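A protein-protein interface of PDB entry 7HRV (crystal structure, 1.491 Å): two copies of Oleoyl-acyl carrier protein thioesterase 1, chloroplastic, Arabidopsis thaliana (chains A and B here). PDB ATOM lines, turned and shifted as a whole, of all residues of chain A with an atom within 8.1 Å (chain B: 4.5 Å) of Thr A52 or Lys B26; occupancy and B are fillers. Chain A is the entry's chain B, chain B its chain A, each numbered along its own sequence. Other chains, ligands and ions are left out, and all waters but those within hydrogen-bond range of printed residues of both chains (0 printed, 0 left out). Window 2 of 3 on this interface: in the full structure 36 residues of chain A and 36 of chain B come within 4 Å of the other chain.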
ATOM      1  N   CYS A  42      -8.508  10.629  -2.466  1.00  0.00           N
ATOM      2  CA  CYS A  42      -9.909  10.750  -2.050  1.00  0.00           C
ATOM      3  C   CYS A  42     -10.349   9.499  -1.264  1.00  0.00           C
ATOM      4  O   CYS A  42     -11.046   9.602  -0.256  1.00  0.00           O
ATOM      5  CB  CYS A  42     -10.804  10.947  -3.271  1.00  0.00           C
ATOM      6  SG  CYS A  42     -10.741  12.613  -3.991  1.00  0.00           S
ATOM      7  N   ALA A  45      -8.876   9.683   2.199  1.00  0.00           N
ATOM      8  CA  ALA A  45      -9.604  10.674   3.034  1.00  0.00           C
ATOM      9  C   ALA A  45     -10.959  10.088   3.521  1.00  0.00           C
ATOM     10  O   ALA A  45     -11.272  10.214   4.691  1.00  0.00           O
ATOM     11  CB  ALA A  45      -9.834  11.967   2.260  1.00  0.00           C
ATOM     12  N   GLN A  46     -11.705   9.385   2.651  1.00  0.00           N
ATOM     13  CA  GLN A  46     -12.973   8.768   3.056  1.00  0.00           C
ATOM     14  C   GLN A  46     -12.743   7.723   4.140  1.00  0.00           C
ATOM     15  O   GLN A  46     -13.547   7.625   5.088  1.00  0.00           O
ATOM     16  CB  GLN A  46     -13.660   8.044   1.867  1.00  0.00           C
ATOM     17  CG  GLN A  46     -14.233   8.937   0.781  1.00  0.00           C
ATOM     18  CD  GLN A  46     -15.077   8.196  -0.249  1.00  0.00           C
ATOM     19  OE1 GLN A  46     -14.925   6.986  -0.523  1.00  0.00           O
ATOM     20  NE2 GLN A  46     -16.008   8.914  -0.860  1.00  0.00           N
ATOM     21  N   SER A  47     -11.673   6.922   3.990  1.00  0.00           N
ATOM     22  CA  SER A  47     -11.374   5.841   4.933  1.00  0.00           C
ATOM     23  C   SER A  47     -11.006   6.336   6.337  1.00  0.00           C
ATOM     24  O   SER A  47     -11.185   5.587   7.310  1.00  0.00           O
ATOM     25  CB  SER A  47     -10.287   4.915   4.394  1.00  0.00           C
ATOM     26  OG  SER A  47      -8.993   5.481   4.509  1.00  0.00           O
ATOM     27  N   GLY A  49     -12.341   9.141   7.780  1.00  0.00           N
ATOM     28  CA  GLY A  49     -13.409   9.996   8.295  1.00  0.00           C
ATOM     29  C   GLY A  49     -13.622  11.402   7.777  1.00  0.00           C
ATOM     30  O   GLY A  49     -14.343  12.174   8.419  1.00  0.00           O
ATOM     31  N   PHE A  50     -13.049  11.758   6.623  1.00  0.00           N
ATOM     32  CA  PHE A  50     -13.236  13.107   6.074  1.00  0.00           C
ATOM     33  C   PHE A  50     -14.620  13.296   5.439  1.00  0.00           C
ATOM     34  O   PHE A  50     -15.326  12.308   5.192  1.00  0.00           O
ATOM     35  CB  PHE A  50     -12.157  13.431   5.046  1.00  0.00           C
ATOM     36  CG  PHE A  50     -10.836  13.873   5.601  1.00  0.00           C
ATOM     37  CD1 PHE A  50      -9.944  12.955   6.114  1.00  0.00           C
ATOM     38  CD2 PHE A  50     -10.419  15.188   5.472  1.00  0.00           C
ATOM     39  CE1 PHE A  50      -8.695  13.356   6.557  1.00  0.00           C
ATOM     40  CE2 PHE A  50      -9.169  15.586   5.917  1.00  0.00           C
ATOM     41  CZ  PHE A  50      -8.317  14.668   6.461  1.00  0.00           C
ATOM     42  N   SER A  51     -14.996  14.572   5.168  1.00  0.00           N
ATOM     43  CA  SER A  51     -16.243  14.944   4.492  1.00  0.00           C
ATOM     44  C   SER A  51     -16.394  14.201   3.165  1.00  0.00           C
ATOM     45  O   SER A  51     -15.420  14.083   2.428  1.00  0.00           O
ATOM     46  CB  SER A  51     -16.225  16.430   4.151  1.00  0.00           C
ATOM     47  OG  SER A  51     -16.718  17.220   5.217  1.00  0.00           O
ATOM     48  N   THR A  52     -17.613  13.760   2.835  1.00  0.00           N
ATOM     49  CA  THR A  52     -17.879  13.106   1.548  1.00  0.00           C
ATOM     50  C   THR A  52     -18.641  14.040   0.586  1.00  0.00           C
ATOM     51  O   THR A  52     -19.433  13.576  -0.231  1.00  0.00           O
ATOM     52  CB  THR A  52     -18.620  11.796   1.782  1.00  0.00           C
ATOM     53  OG1 THR A  52     -19.875  12.084   2.408  1.00  0.00           O
ATOM     54  CG2 THR A  52     -17.820  10.837   2.659  1.00  0.00           C
ATOM     55  N   ASP A  53     -18.410  15.357   0.694  1.00  0.00           N
ATOM     56  CA  ASP A  53     -19.089  16.338  -0.150  1.00  0.00           C
ATOM     57  C   ASP A  53     -18.218  16.904  -1.286  1.00  0.00           C
ATOM     58  O   ASP A  53     -18.664  17.809  -1.985  1.00  0.00           O
ATOM     59  CB  ASP A  53     -19.619  17.493   0.716  1.00  0.00           C
ATOM     60  CG  ASP A  53     -18.568  18.127   1.620  1.00  0.00           C
ATOM     61  OD1 ASP A  53     -17.355  17.889   1.388  1.00  0.00           O
ATOM     62  OD2 ASP A  53     -18.958  18.861   2.563  1.00  0.00           O
ATOM     63  N   GLY A  54     -16.997  16.394  -1.443  1.00  0.00           N
ATOM     64  CA  GLY A  54     -16.074  16.865  -2.468  1.00  0.00           C
ATOM     65  C   GLY A  54     -14.999  17.801  -1.956  1.00  0.00           C
ATOM     66  O   GLY A  54     -14.005  18.038  -2.650  1.00  0.00           O
ATOM     67  N   PHE A  55     -15.187  18.354  -0.738  1.00  0.00           N
ATOM     68  CA  PHE A  55     -14.232  19.295  -0.159  1.00  0.00           C
ATOM     69  C   PHE A  55     -13.177  18.644   0.742  1.00  0.00           C
ATOM     70  O   PHE A  55     -12.219  19.324   1.124  1.00  0.00           O
ATOM     71  CB  PHE A  55     -14.965  20.418   0.601  1.00  0.00           C
ATOM     72  CG  PHE A  55     -15.952  21.208  -0.222  1.00  0.00           C
ATOM     73  CD1 PHE A  55     -15.516  22.143  -1.145  1.00  0.00           C
ATOM     74  CD2 PHE A  55     -17.315  21.039  -0.052  1.00  0.00           C
ATOM     75  CE1 PHE A  55     -16.427  22.877  -1.896  1.00  0.00           C
ATOM     76  CE2 PHE A  55     -18.223  21.778  -0.798  1.00  0.00           C
ATOM     77  CZ  PHE A  55     -17.773  22.698  -1.712  1.00  0.00           C
ATOM     78  N   ALA A  56     -13.347  17.360   1.113  1.00  0.00           N
ATOM     79  CA  ALA A  56     -12.392  16.636   1.981  1.00  0.00           C
ATOM     80  C   ALA A  56     -11.936  17.457   3.214  1.00  0.00           C
ATOM     81  O   ALA A  56     -10.745  17.693   3.414  1.00  0.00           O
ATOM     82  CB  ALA A  56     -11.185  16.174   1.169  1.00  0.00           C
ATOM     83  N   THR A  57     -12.887  17.915   4.007  1.00  0.00           N
ATOM     84  CA  THR A  57     -12.595  18.740   5.184  1.00  0.00           C
ATOM     85  C   THR A  57     -12.724  17.938   6.487  1.00  0.00           C
ATOM     86  O   THR A  57     -13.484  16.967   6.535  1.00  0.00           O
ATOM     87  CB  THR A  57     -13.661  19.841   5.272  1.00  0.00           C
ATOM     88  OG1 THR A  57     -14.940  19.205   5.334  1.00  0.00           O
ATOM     89  CG2 THR A  57     -13.618  20.793   4.096  1.00  0.00           C
ATOM     90  N   ARG A  62     -14.934  22.377   8.869  1.00  0.00           N
ATOM     91  CA  ARG A  62     -16.323  22.703   8.505  1.00  0.00           C
ATOM     92  C   ARG A  62     -16.889  23.811   9.392  1.00  0.00           C
ATOM     93  O   ARG A  62     -17.468  24.780   8.879  1.00  0.00           O
ATOM     94  CB  ARG A  62     -17.225  21.468   8.576  1.00  0.00           C
ATOM     95  CG  ARG A  62     -16.930  20.502   7.460  1.00  0.00           C
ATOM     96  CD  ARG A  62     -17.987  19.411   7.353  1.00  0.00           C
ATOM     97  NE  ARG A  62     -18.006  18.501   8.500  1.00  0.00           N
ATOM     98  CZ  ARG A  62     -17.165  17.486   8.674  1.00  0.00           C
ATOM     99  NH1 ARG A  62     -16.205  17.251   7.787  1.00  0.00           N
ATOM    100  NH2 ARG A  62     -17.276  16.698   9.738  1.00  0.00           N
ATOM    101  N   MET A 190     -16.870  17.806  -8.762  1.00  0.00           N
ATOM    102  CA  MET A 190     -18.251  17.794  -8.292  1.00  0.00           C
ATOM    103  C   MET A 190     -18.663  19.139  -7.642  1.00  0.00           C
ATOM    104  O   MET A 190     -19.850  19.441  -7.591  1.00  0.00           O
ATOM    105  CB  MET A 190     -18.458  16.608  -7.339  1.00  0.00           C
ATOM    106  CG  MET A 190     -17.630  16.716  -6.088  1.00  0.00           C
ATOM    107  SD  MET A 190     -17.858  15.228  -5.055  1.00  0.00           S
ATOM    108  CE  MET A 190     -16.572  14.134  -5.786  1.00  0.00           C
ATOM    109  N   ASN A 191     -17.694  19.970  -7.214  1.00  0.00           N
ATOM    110  CA  ASN A 191     -18.023  21.286  -6.636  1.00  0.00           C
ATOM    111  C   ASN A 191     -17.948  22.441  -7.665  1.00  0.00           C
ATOM    112  O   ASN A 191     -18.049  23.615  -7.296  1.00  0.00           O
ATOM    113  CB  ASN A 191     -17.149  21.565  -5.428  1.00  0.00           C
ATOM    114  CG  ASN A 191     -17.304  20.517  -4.358  1.00  0.00           C
ATOM    115  OD1 ASN A 191     -16.321  19.987  -3.848  1.00  0.00           O
ATOM    116  ND2 ASN A 191     -18.545  20.182  -4.006  1.00  0.00           N
ATOM    117  N   VAL B  22     -17.683  12.179 -11.480  1.00  0.00           N
ATOM    118  CA  VAL B  22     -19.023  12.607 -11.123  1.00  0.00           C
ATOM    119  C   VAL B  22     -19.234  14.090 -11.273  1.00  0.00           C
ATOM    120  O   VAL B  22     -18.280  14.873 -11.169  1.00  0.00           O
ATOM    121  CB  VAL B  22     -19.427  12.125  -9.690  1.00  0.00           C
ATOM    122  CG1 VAL B  22     -19.218  10.628  -9.540  1.00  0.00           C
ATOM    123  CG2 VAL B  22     -18.663  12.874  -8.622  1.00  0.00           C
ATOM    124  N   GLY B  23     -20.500  14.463 -11.479  1.00  0.00           N
ATOM    125  CA  GLY B  23     -20.903  15.867 -11.590  1.00  0.00           C
ATOM    126  C   GLY B  23     -21.413  16.450 -10.283  1.00  0.00           C
ATOM    127  O   GLY B  23     -21.141  15.897  -9.216  1.00  0.00           O
ATOM    128  N   SER B  24     -22.159  17.576 -10.354  1.00  0.00           N
ATOM    129  CA  SER B  24     -22.666  18.276  -9.170  1.00  0.00           C
ATOM    130  C   SER B  24     -23.580  17.449  -8.255  1.00  0.00           C
ATOM    131  O   SER B  24     -23.584  17.689  -7.046  1.00  0.00           O
ATOM    132  CB  SER B  24     -23.359  19.579  -9.557  1.00  0.00           C
ATOM    133  OG  SER B  24     -24.624  19.331 -10.143  1.00  0.00           O
ATOM    134  N   ASN B  25     -24.334  16.473  -8.802  1.00  0.00           N
ATOM    135  CA  ASN B  25     -25.194  15.630  -7.947  1.00  0.00           C
ATOM    136  C   ASN B  25     -24.459  14.390  -7.392  1.00  0.00           C
ATOM    137  O   ASN B  25     -25.102  13.451  -6.911  1.00  0.00           O
ATOM    138  CB  ASN B  25     -26.455  15.194  -8.655  1.00  0.00           C
ATOM    139  CG  ASN B  25     -27.189  16.352  -9.272  1.00  0.00           C
ATOM    140  OD1 ASN B  25     -27.076  16.590 -10.478  1.00  0.00           O
ATOM    141  ND2 ASN B  25     -27.917  17.124  -8.455  1.00  0.00           N
ATOM    142  N   LYS B  26     -23.118  14.371  -7.492  1.00  0.00           N
ATOM    143  CA  LYS B  26     -22.302  13.262  -7.029  1.00  0.00           C
ATOM    144  C   LYS B  26     -22.643  11.957  -7.744  1.00  0.00           C
ATOM    145  O   LYS B  26     -22.391  10.899  -7.193  1.00  0.00           O
ATOM    146  CB  LYS B  26     -22.306  13.095  -5.489  1.00  0.00           C
ATOM    147  CG  LYS B  26     -21.602  14.244  -4.746  1.00  0.00           C
ATOM    148  CD  LYS B  26     -21.655  14.067  -3.228  1.00  0.00           C
ATOM    149  CE  LYS B  26     -21.293  15.350  -2.507  1.00  0.00           C
ATOM    150  NZ  LYS B  26     -22.233  15.650  -1.380  1.00  0.00           N
ATOM    151  N   THR B  27     -23.155  12.025  -9.000  1.00  0.00           N
ATOM    152  CA  THR B  27     -23.376  10.818  -9.798  1.00  0.00           C
ATOM    153  C   THR B  27     -22.543  10.928 -11.096  1.00  0.00           C
ATOM    154  O   THR B  27     -22.168  12.035 -11.523  1.00  0.00           O
ATOM    155  CB  THR B  27     -24.864  10.563 -10.094  1.00  0.00           C
ATOM    156  OG1 THR B  27     -25.379  11.644 -10.848  1.00  0.00           O
ATOM    157  CG2 THR B  27     -25.710  10.349  -8.800  1.00  0.00           C
ATOM    158  N   ALA B  82     -23.834   6.569  -8.306  1.00  0.00           N
ATOM    159  CA  ALA B  82     -23.200   7.567  -7.442  1.00  0.00           C
ATOM    160  C   ALA B  82     -21.696   7.265  -7.301  1.00  0.00           C
ATOM    161  O   ALA B  82     -21.255   6.154  -7.513  1.00  0.00           O
ATOM    162  CB  ALA B  82     -23.858   7.534  -6.060  1.00  0.00           C
ATOM    163  N   TRP B  83     -20.923   8.272  -6.896  1.00  0.00           N
ATOM    164  CA  TRP B  83     -19.508   8.175  -6.543  1.00  0.00           C
ATOM    165  C   TRP B  83     -19.294   6.965  -5.553  1.00  0.00           C
ATOM    166  O   TRP B  83     -20.014   6.877  -4.546  1.00  0.00           O
ATOM    167  CB  TRP B  83     -19.185   9.504  -5.839  1.00  0.00           C
ATOM    168  CG  TRP B  83     -17.831   9.631  -5.226  1.00  0.00           C
ATOM    169  CD1 TRP B  83     -16.711   8.903  -5.509  1.00  0.00           C
ATOM    170  CD2 TRP B  83     -17.435  10.629  -4.276  1.00  0.00           C
ATOM    171  NE1 TRP B  83     -15.654   9.352  -4.756  1.00  0.00           N
ATOM    172  CE2 TRP B  83     -16.077  10.400  -3.969  1.00  0.00           C
ATOM    173  CE3 TRP B  83     -18.113  11.662  -3.617  1.00  0.00           C
ATOM    174  CZ2 TRP B  83     -15.367  11.217  -3.085  1.00  0.00           C
ATOM    175  CZ3 TRP B  83     -17.415  12.455  -2.723  1.00  0.00           C
ATOM    176  CH2 TRP B  83     -16.056  12.239  -2.475  1.00  0.00           C
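The backbone carbonyl oxygen of Asp A53 is in hydrogen-bond range of the side-chain amide nitrogen of Asn A191 (3.1 Å).
The backbone NH of Trp B83 lies within hydrogen-bond range of the backbone carbonyl oxygen of Lys B26.
The side-chain carboxylate of Asp A53 lies within hydrogen-bond range of the backbone NH of Phe A55, at 3.1 Å.
Among the printed residues, merely in contact across the chains: Gln A46 with Trp B83, Thr A52 with Lys B26, Thr A52 with Trp B83, Asp A53 with Lys B26, Met A190 with Val B22, Met A190 with Gly B23, Met A190 with Ser B24, Met A190 with Lys B26 and Met A190 with Trp B83.
Of chain B, only Lys B26 and Trp B83 come within 4 Å of Thr A52.
Printed residues of chain A within 4 Å of Gly B23: Met A190 (3.4 Å).
Lys B26 touches just these residues of chain A: Thr A52 (3.4 Å), Asp A53 (3.4 Å) and Met A190 (3.9 Å).
Printed residues of chain A within 4 Å of Trp B83: Gln A46, Thr A52 and Met A190.
The nearest printed residue of chain B that does not touch Thr A52 is Val B22 (8.5 Å).
The nearest residue of chain A that does not touch Lys B26 is Gly A54 (4.5 Å).
The nearest printed residue of chain B that does not touch Gln A46 is Lys B26 (8.0 Å).
Hydrophobic or aromatic side chains of chain A that line the printed part of chain B: Met A190.
Among the printed residues, 9 pairs touch across the chains.
No position is printed for both chains.
Of the 9 pairs that touch across the chains among the printed residues, none has its exchanged pair printed and touching as well.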
